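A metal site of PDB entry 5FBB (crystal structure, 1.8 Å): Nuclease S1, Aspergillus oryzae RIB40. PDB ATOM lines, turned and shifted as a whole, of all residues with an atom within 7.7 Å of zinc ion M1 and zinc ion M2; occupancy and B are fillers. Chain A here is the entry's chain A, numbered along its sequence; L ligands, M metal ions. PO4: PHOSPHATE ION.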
ATOM      1  N   TRP A   1     -11.481   9.036  27.017  1.00  0.00           N
ATOM      2  CA  TRP A   1     -11.146   9.902  28.152  1.00  0.00           C
ATOM      3  C   TRP A   1     -11.571  11.294  27.825  1.00  0.00           C
ATOM      4  O   TRP A   1     -11.721  11.656  26.643  1.00  0.00           O
ATOM      5  CB  TRP A   1      -9.596   9.923  28.420  1.00  0.00           C
ATOM      6  CG  TRP A   1      -8.944   8.513  28.572  1.00  0.00           C
ATOM      7  CD1 TRP A   1      -8.257   7.832  27.603  1.00  0.00           C
ATOM      8  CD2 TRP A   1      -8.994   7.650  29.706  1.00  0.00           C
ATOM      9  NE1 TRP A   1      -7.865   6.629  28.073  1.00  0.00           N
ATOM     10  CE2 TRP A   1      -8.316   6.484  29.369  1.00  0.00           C
ATOM     11  CE3 TRP A   1      -9.596   7.737  30.971  1.00  0.00           C
ATOM     12  CZ2 TRP A   1      -8.165   5.416  30.236  1.00  0.00           C
ATOM     13  CZ3 TRP A   1      -9.487   6.666  31.843  1.00  0.00           C
ATOM     14  CH2 TRP A   1      -8.765   5.531  31.476  1.00  0.00           C
ATOM     15  N   GLY A   2     -11.685  12.116  28.873  1.00  0.00           N
ATOM     16  CA  GLY A   2     -11.833  13.533  28.712  1.00  0.00           C
ATOM     17  C   GLY A   2     -10.477  14.162  28.517  1.00  0.00           C
ATOM     18  O   GLY A   2      -9.443  13.459  28.325  1.00  0.00           O
ATOM     19  N   ASN A   3     -10.398  15.483  28.641  1.00  0.00           N
ATOM     20  CA  ASN A   3      -9.193  16.201  28.196  1.00  0.00           C
ATOM     21  C   ASN A   3      -7.957  15.850  28.991  1.00  0.00           C
ATOM     22  O   ASN A   3      -6.896  15.644  28.395  1.00  0.00           O
ATOM     23  CB  ASN A   3      -9.380  17.734  28.202  1.00  0.00           C
ATOM     24  CG  ASN A   3     -10.396  18.182  27.177  1.00  0.00           C
ATOM     25  OD1 ASN A   3     -10.944  17.370  26.377  1.00  0.00           O
ATOM     26  ND2 ASN A   3     -10.613  19.477  27.111  1.00  0.00           N
ATOM     27  N   GLY A   5      -7.225  13.145  30.581  1.00  0.00           N
ATOM     28  CA  GLY A   5      -6.810  11.801  30.224  1.00  0.00           C
ATOM     29  C   GLY A   5      -5.982  11.773  28.954  1.00  0.00           C
ATOM     30  O   GLY A   5      -4.881  11.191  28.925  1.00  0.00           O
ATOM     31  N   HIS A   6      -6.469  12.442  27.913  1.00  0.00           N
ATOM     32  CA  HIS A   6      -5.755  12.545  26.628  1.00  0.00           C
ATOM     33  C   HIS A   6      -4.463  13.281  26.680  1.00  0.00           C
ATOM     34  O   HIS A   6      -3.470  12.837  26.068  1.00  0.00           O
ATOM     35  CB  HIS A   6      -6.640  13.138  25.555  1.00  0.00           C
ATOM     36  CG  HIS A   6      -7.693  12.181  25.122  1.00  0.00           C
ATOM     37  ND1 HIS A   6      -7.374  11.023  24.434  1.00  0.00           N
ATOM     38  CD2 HIS A   6      -9.001  12.098  25.414  1.00  0.00           C
ATOM     39  CE1 HIS A   6      -8.474  10.329  24.231  1.00  0.00           C
ATOM     40  NE2 HIS A   6      -9.466  10.931  24.864  1.00  0.00           N
ATOM     41  N   ALA A  41      -3.888  16.615  21.581  1.00  0.00           N
ATOM     42  CA  ALA A  41      -4.422  15.327  22.056  1.00  0.00           C
ATOM     43  C   ALA A  41      -5.919  15.322  22.196  1.00  0.00           C
ATOM     44  O   ALA A  41      -6.533  14.216  22.301  1.00  0.00           O
ATOM     45  CB  ALA A  41      -3.793  14.896  23.353  1.00  0.00           C
ATOM     46  N   THR A  42      -6.525  16.502  22.274  1.00  0.00           N
ATOM     47  CA  THR A  42      -7.976  16.626  22.428  1.00  0.00           C
ATOM     48  C   THR A  42      -8.717  17.039  21.135  1.00  0.00           C
ATOM     49  O   THR A  42      -9.960  17.004  21.098  1.00  0.00           O
ATOM     50  CB  THR A  42      -8.331  17.703  23.487  1.00  0.00           C
ATOM     51  OG1 THR A  42      -7.891  18.982  23.029  1.00  0.00           O
ATOM     52  CG2 THR A  42      -7.645  17.409  24.767  1.00  0.00           C
ATOM     53  N   ALA A  44      -9.397  15.689  18.198  1.00  0.00           N
ATOM     54  CA  ALA A  44     -10.386  14.790  17.641  1.00  0.00           C
ATOM     55  C   ALA A  44     -11.726  14.887  18.335  1.00  0.00           C
ATOM     56  O   ALA A  44     -12.757  14.643  17.703  1.00  0.00           O
ATOM     57  CB  ALA A  44      -9.876  13.336  17.653  1.00  0.00           C
ATOM     58  N   ASP A  45     -11.733  15.180  19.640  1.00  0.00           N
ATOM     59  CA  ASP A  45     -12.965  15.368  20.407  1.00  0.00           C
ATOM     60  C   ASP A  45     -13.731  16.605  20.002  1.00  0.00           C
ATOM     61  O   ASP A  45     -14.952  16.583  20.027  1.00  0.00           O
ATOM     62  CB  ASP A  45     -12.793  15.318  21.913  1.00  0.00           C
ATOM     63  CG  ASP A  45     -12.791  13.845  22.484  1.00  0.00           C
ATOM     64  OD1 ASP A  45     -13.132  12.879  21.729  1.00  0.00           O
ATOM     65  OD2 ASP A  45     -12.424  13.688  23.725  1.00  0.00           O
ATOM     66  N   THR A  46     -13.065  17.670  19.624  1.00  0.00           N
ATOM     67  CA  THR A  46     -13.769  18.828  18.997  1.00  0.00           C
ATOM     68  C   THR A  46     -14.304  18.476  17.633  1.00  0.00           C
ATOM     69  O   THR A  46     -15.457  18.750  17.311  1.00  0.00           O
ATOM     70  CB  THR A  46     -12.818  20.016  18.861  1.00  0.00           C
ATOM     71  OG1 THR A  46     -12.521  20.494  20.160  1.00  0.00           O
ATOM     72  CG2 THR A  46     -13.411  21.164  17.996  1.00  0.00           C
ATOM     73  N   LYS A  48     -15.187  15.794  16.093  1.00  0.00           N
ATOM     74  CA  LYS A  48     -16.304  14.907  15.935  1.00  0.00           C
ATOM     75  C   LYS A  48     -17.667  15.594  16.147  1.00  0.00           C
ATOM     76  O   LYS A  48     -18.714  14.996  15.778  1.00  0.00           O
ATOM     77  CB  LYS A  48     -16.191  13.682  16.837  1.00  0.00           C
ATOM     78  CG  LYS A  48     -16.509  13.939  18.272  1.00  0.00           C
ATOM     79  CD  LYS A  48     -16.146  12.772  19.133  1.00  0.00           C
ATOM     80  CE  LYS A  48     -16.597  12.901  20.561  1.00  0.00           C
ATOM     81  NZ  LYS A  48     -16.175  11.693  21.305  1.00  0.00           N
ATOM     82  N   SER A  56     -16.071  11.032  11.864  1.00  0.00           N
ATOM     83  CA  SER A  56     -15.078  10.485  12.750  1.00  0.00           C
ATOM     84  C   SER A  56     -15.585  10.127  14.151  1.00  0.00           C
ATOM     85  O   SER A  56     -14.847   9.561  14.946  1.00  0.00           O
ATOM     86  CB  SER A  56     -13.884  11.441  12.814  1.00  0.00           C
ATOM     87  OG  SER A  56     -14.216  12.619  13.558  1.00  0.00           O
ATOM     88  N   LYS A  57     -16.857  10.370  14.425  1.00  0.00           N
ATOM     89  CA  LYS A  57     -17.416  10.026  15.742  1.00  0.00           C
ATOM     90  C   LYS A  57     -17.227   8.562  16.126  1.00  0.00           C
ATOM     91  O   LYS A  57     -16.839   8.265  17.263  1.00  0.00           O
ATOM     92  CB  LYS A  57     -18.912  10.336  15.831  1.00  0.00           C
ATOM     93  CG  LYS A  57     -19.261  11.781  16.105  1.00  0.00           C
ATOM     94  CD  LYS A  57     -20.767  11.963  16.259  1.00  0.00           C
ATOM     95  CE  LYS A  57     -21.306  11.250  17.518  1.00  0.00           C
ATOM     96  NZ  LYS A  57     -20.737  11.740  18.861  1.00  0.00           N
ATOM     97  N   TYR A  59     -14.870   6.633  15.387  1.00  0.00           N
ATOM     98  CA  TYR A  59     -13.459   6.281  15.468  1.00  0.00           C
ATOM     99  C   TYR A  59     -12.918   6.317  16.916  1.00  0.00           C
ATOM    100  O   TYR A  59     -11.808   5.933  17.128  1.00  0.00           O
ATOM    101  CB  TYR A  59     -12.635   7.160  14.617  1.00  0.00           C
ATOM    102  CG  TYR A  59     -12.925   7.151  13.133  1.00  0.00           C
ATOM    103  CD1 TYR A  59     -13.843   6.300  12.537  1.00  0.00           C
ATOM    104  CD2 TYR A  59     -12.253   8.052  12.325  1.00  0.00           C
ATOM    105  CE1 TYR A  59     -14.108   6.394  11.161  1.00  0.00           C
ATOM    106  CE2 TYR A  59     -12.526   8.129  10.982  1.00  0.00           C
ATOM    107  CZ  TYR A  59     -13.411   7.249  10.397  1.00  0.00           C
ATOM    108  OH  TYR A  59     -13.660   7.329   9.027  1.00  0.00           O
ATOM    109  N   HIS A  60     -13.732   6.742  17.883  1.00  0.00           N
ATOM    110  CA  HIS A  60     -13.326   6.831  19.298  1.00  0.00           C
ATOM    111  C   HIS A  60     -13.480   5.544  20.085  1.00  0.00           C
ATOM    112  O   HIS A  60     -13.068   5.487  21.230  1.00  0.00           O
ATOM    113  CB  HIS A  60     -14.006   8.025  20.001  1.00  0.00           C
ATOM    114  CG  HIS A  60     -13.662   9.344  19.364  1.00  0.00           C
ATOM    115  ND1 HIS A  60     -12.890  10.312  19.985  1.00  0.00           N
ATOM    116  CD2 HIS A  60     -13.895   9.798  18.108  1.00  0.00           C
ATOM    117  CE1 HIS A  60     -12.680  11.301  19.153  1.00  0.00           C
ATOM    118  NE2 HIS A  60     -13.262  11.021  18.004  1.00  0.00           N
ATOM    119  N   PHE A  61     -14.163   4.560  19.492  1.00  0.00           N
ATOM    120  CA  PHE A  61     -14.511   3.391  20.244  1.00  0.00           C
ATOM    121  C   PHE A  61     -14.711   2.177  19.355  1.00  0.00           C
ATOM    122  O   PHE A  61     -14.723   2.244  18.151  1.00  0.00           O
ATOM    123  CB  PHE A  61     -15.752   3.655  21.149  1.00  0.00           C
ATOM    124  CG  PHE A  61     -16.938   4.094  20.366  1.00  0.00           C
ATOM    125  CD1 PHE A  61     -17.780   3.166  19.746  1.00  0.00           C
ATOM    126  CD2 PHE A  61     -17.234   5.442  20.235  1.00  0.00           C
ATOM    127  CE1 PHE A  61     -18.868   3.600  18.980  1.00  0.00           C
ATOM    128  CE2 PHE A  61     -18.274   5.872  19.427  1.00  0.00           C
ATOM    129  CZ  PHE A  61     -19.091   4.963  18.807  1.00  0.00           C
ATOM    130  N   HIS A 115      -4.833  10.726  19.849  1.00  0.00           N
ATOM    131  CA  HIS A 115      -6.104  10.657  20.609  1.00  0.00           C
ATOM    132  C   HIS A 115      -6.672   9.260  20.748  1.00  0.00           C
ATOM    133  O   HIS A 115      -6.971   8.794  21.864  1.00  0.00           O
ATOM    134  CB  HIS A 115      -7.119  11.591  19.973  1.00  0.00           C
ATOM    135  CG  HIS A 115      -8.405  11.652  20.705  1.00  0.00           C
ATOM    136  ND1 HIS A 115      -8.672  12.618  21.636  1.00  0.00           N
ATOM    137  CD2 HIS A 115      -9.502  10.856  20.656  1.00  0.00           C
ATOM    138  CE1 HIS A 115      -9.863  12.428  22.154  1.00  0.00           C
ATOM    139  NE2 HIS A 115     -10.404  11.385  21.556  1.00  0.00           N
ATOM    140  N   ILE A 116      -6.707   8.562  19.630  1.00  0.00           N
ATOM    141  CA  ILE A 116      -7.406   7.271  19.561  1.00  0.00           C
ATOM    142  C   ILE A 116      -6.634   6.214  20.314  1.00  0.00           C
ATOM    143  O   ILE A 116      -7.249   5.365  20.988  1.00  0.00           O
ATOM    144  CB  ILE A 116      -7.743   6.874  18.125  1.00  0.00           C
ATOM    145  CG1 ILE A 116      -8.690   7.904  17.514  1.00  0.00           C
ATOM    146  CG2 ILE A 116      -8.311   5.451  18.125  1.00  0.00           C
ATOM    147  CD1 ILE A 116      -8.983   7.677  16.041  1.00  0.00           C
ATOM    148  N   GLY A 118      -5.211   6.738  22.993  1.00  0.00           N
ATOM    149  CA  GLY A 118      -5.681   6.987  24.362  1.00  0.00           C
ATOM    150  C   GLY A 118      -7.056   6.325  24.540  1.00  0.00           C
ATOM    151  O   GLY A 118      -7.302   5.635  25.565  1.00  0.00           O
ATOM    152  N   ASP A 119      -7.983   6.617  23.675  1.00  0.00           N
ATOM    153  CA  ASP A 119      -9.371   6.112  23.808  1.00  0.00           C
ATOM    154  C   ASP A 119      -9.487   4.594  23.862  1.00  0.00           C
ATOM    155  O   ASP A 119     -10.285   4.080  24.645  1.00  0.00           O
ATOM    156  CB  ASP A 119     -10.326   6.611  22.722  1.00  0.00           C
ATOM    157  CG  ASP A 119     -10.911   7.964  23.016  1.00  0.00           C
ATOM    158  OD1 ASP A 119     -10.866   8.423  24.214  1.00  0.00           O
ATOM    159  OD2 ASP A 119     -11.409   8.616  22.048  1.00  0.00           O
ATOM    160  N   ILE A 120      -8.614   3.904  23.144  1.00  0.00           N
ATOM    161  CA  ILE A 120      -8.576   2.454  23.117  1.00  0.00           C
ATOM    162  C   ILE A 120      -8.348   1.919  24.533  1.00  0.00           C
ATOM    163  O   ILE A 120      -8.854   0.843  24.856  1.00  0.00           O
ATOM    164  CB  ILE A 120      -7.597   1.927  22.075  1.00  0.00           C
ATOM    165  CG1 ILE A 120      -8.158   2.150  20.685  1.00  0.00           C
ATOM    166  CG2 ILE A 120      -7.329   0.443  22.269  1.00  0.00           C
ATOM    167  CD1 ILE A 120      -7.123   1.921  19.531  1.00  0.00           C
ATOM    168  N   GLN A 122      -9.410   3.302  27.427  1.00  0.00           N
ATOM    169  CA  GLN A 122     -10.523   3.544  28.318  1.00  0.00           C
ATOM    170  C   GLN A 122     -11.435   2.331  28.135  1.00  0.00           C
ATOM    171  O   GLN A 122     -11.997   2.170  27.080  1.00  0.00           O
ATOM    172  CB  GLN A 122     -11.190   4.868  27.984  1.00  0.00           C
ATOM    173  CG  GLN A 122     -11.913   5.541  29.144  1.00  0.00           C
ATOM    174  CD  GLN A 122     -13.243   4.902  29.562  1.00  0.00           C
ATOM    175  OE1 GLN A 122     -13.314   3.728  29.907  1.00  0.00           O
ATOM    176  NE2 GLN A 122     -14.318   5.728  29.568  1.00  0.00           N
ATOM    177  N   HIS A 125     -14.712   2.522  26.210  1.00  0.00           N
ATOM    178  CA  HIS A 125     -14.588   2.734  24.784  1.00  0.00           C
ATOM    179  C   HIS A 125     -14.400   1.408  24.014  1.00  0.00           C
ATOM    180  O   HIS A 125     -14.211   1.407  22.775  1.00  0.00           O
ATOM    181  CB  HIS A 125     -13.386   3.694  24.518  1.00  0.00           C
ATOM    182  CG  HIS A 125     -13.731   5.138  24.742  1.00  0.00           C
ATOM    183  ND1 HIS A 125     -13.758   6.059  23.728  1.00  0.00           N
ATOM    184  CD2 HIS A 125     -14.102   5.800  25.871  1.00  0.00           C
ATOM    185  CE1 HIS A 125     -14.127   7.230  24.199  1.00  0.00           C
ATOM    186  NE2 HIS A 125     -14.350   7.106  25.508  1.00  0.00           N
ATOM    187  N   HIS A 148     -19.960   6.090  32.129  1.00  0.00           N
ATOM    188  CA  HIS A 148     -18.942   6.477  31.139  1.00  0.00           C
ATOM    189  C   HIS A 148     -18.174   7.724  31.570  1.00  0.00           C
ATOM    190  O   HIS A 148     -16.951   7.804  31.513  1.00  0.00           O
ATOM    191  CB  HIS A 148     -19.584   6.703  29.787  1.00  0.00           C
ATOM    192  CG  HIS A 148     -18.580   6.818  28.694  1.00  0.00           C
ATOM    193  ND1 HIS A 148     -18.220   5.747  27.903  1.00  0.00           N
ATOM    194  CD2 HIS A 148     -17.781   7.839  28.338  1.00  0.00           C
ATOM    195  CE1 HIS A 148     -17.282   6.134  27.065  1.00  0.00           C
ATOM    196  NE2 HIS A 148     -17.007   7.393  27.307  1.00  0.00           N
ATOM    197  N   ASP A 152     -14.283   8.532  32.088  1.00  0.00           N
ATOM    198  CA  ASP A 152     -13.596   9.540  31.251  1.00  0.00           C
ATOM    199  C   ASP A 152     -12.940  10.691  32.022  1.00  0.00           C
ATOM    200  O   ASP A 152     -11.857  11.182  31.633  1.00  0.00           O
ATOM    201  CB  ASP A 152     -14.560  10.185  30.236  1.00  0.00           C
ATOM    202  CG  ASP A 152     -14.666   9.396  28.866  1.00  0.00           C
ATOM    203  OD1 ASP A 152     -13.905   8.418  28.589  1.00  0.00           O
ATOM    204  OD2 ASP A 152     -15.483   9.863  28.057  1.00  0.00           O
HETATM  205  P   PO4 L   1     -14.020  10.732  24.412  1.00  0.00           P
HETATM  206  O1  PO4 L   1     -14.072  10.020  25.753  1.00  0.00           O
HETATM  207  O2  PO4 L   1     -14.889  10.283  23.228  1.00  0.00           O
HETATM  208  O3  PO4 L   1     -12.625  10.736  23.738  1.00  0.00           O
HETATM  209  O4  PO4 L   1     -14.471  12.189  24.791  1.00  0.00           O
HETATM  210 ZN    ZN M   1     -11.344  10.134  25.231  1.00  0.00          ZN
HETATM  211 ZN    ZN M   2     -12.225  10.493  21.942  1.00  0.00          ZN
HETATM  212 ZN    ZN M   3     -15.494   8.644  26.416  1.00  0.00          ZN
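O of His 115 lies close to ND1 of His 6.
ND1 of His 115 lies within hydrogen-bond range of O of Ala 41, at 2.8 Å.
The backbone carbonyl oxygen (O) of His 60 is in hydrogen-bond range of a ring nitrogen (ND1) of His 125, 2.7 Å away.
N of Trp 1 lies close to OD1 of Asp 152 (3.0 Å).
O of Gly 118 sits at hydrogen-bond distance from NE1 of Trp 1.
OD1 of Asp 45 sits close to NZ of Lys 48.
Of the 25 residues printed, 4 come within 4 Å of zinc ion M1.
The nearest printed residue that does not touch zinc ion M1 is Asp 45 (4.01 Å).
Four residues have an atom within 4 Å of zinc ion M2: Asp 45, His 60, His 115 and Asp 119.
Along chain A the residues within 4 Å of zinc ion M2 span positions 45 to 119.
Zinc ion M1 is bound by the side-chain carboxylate (OD1) of Asp 119 (2.0 Å), an oxygen (O3) of the ligand (2.1 Å), a ring nitrogen (NE2) of His 6 (2.1 Å), the backbone nitrogen (N) of Trp 1 (2.1 Å) and the backbone carbonyl oxygen (O) of Trp 1 (2.1 Å).
Zinc ion M1 has five donor atoms within binding distance.
Slightly farther from zinc ion M1 lies an oxygen (O1) of the ligand (2.8 Å).
O3 of the ligand binds zinc ion M2.
The side-chain carboxylate (OD2) of Asp 119 binds zinc ion M2.
Zinc ion M2 is bound by a ring nitrogen (NE2) of His 115, 2.1 Å away.
Zinc ion M2 is bound by a ring nitrogen (ND1) of His 60, 2.1 Å away.
Zinc ion M2 is bound by the side-chain carboxylate (OD1) of Asp 45, at 2.6 Å.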
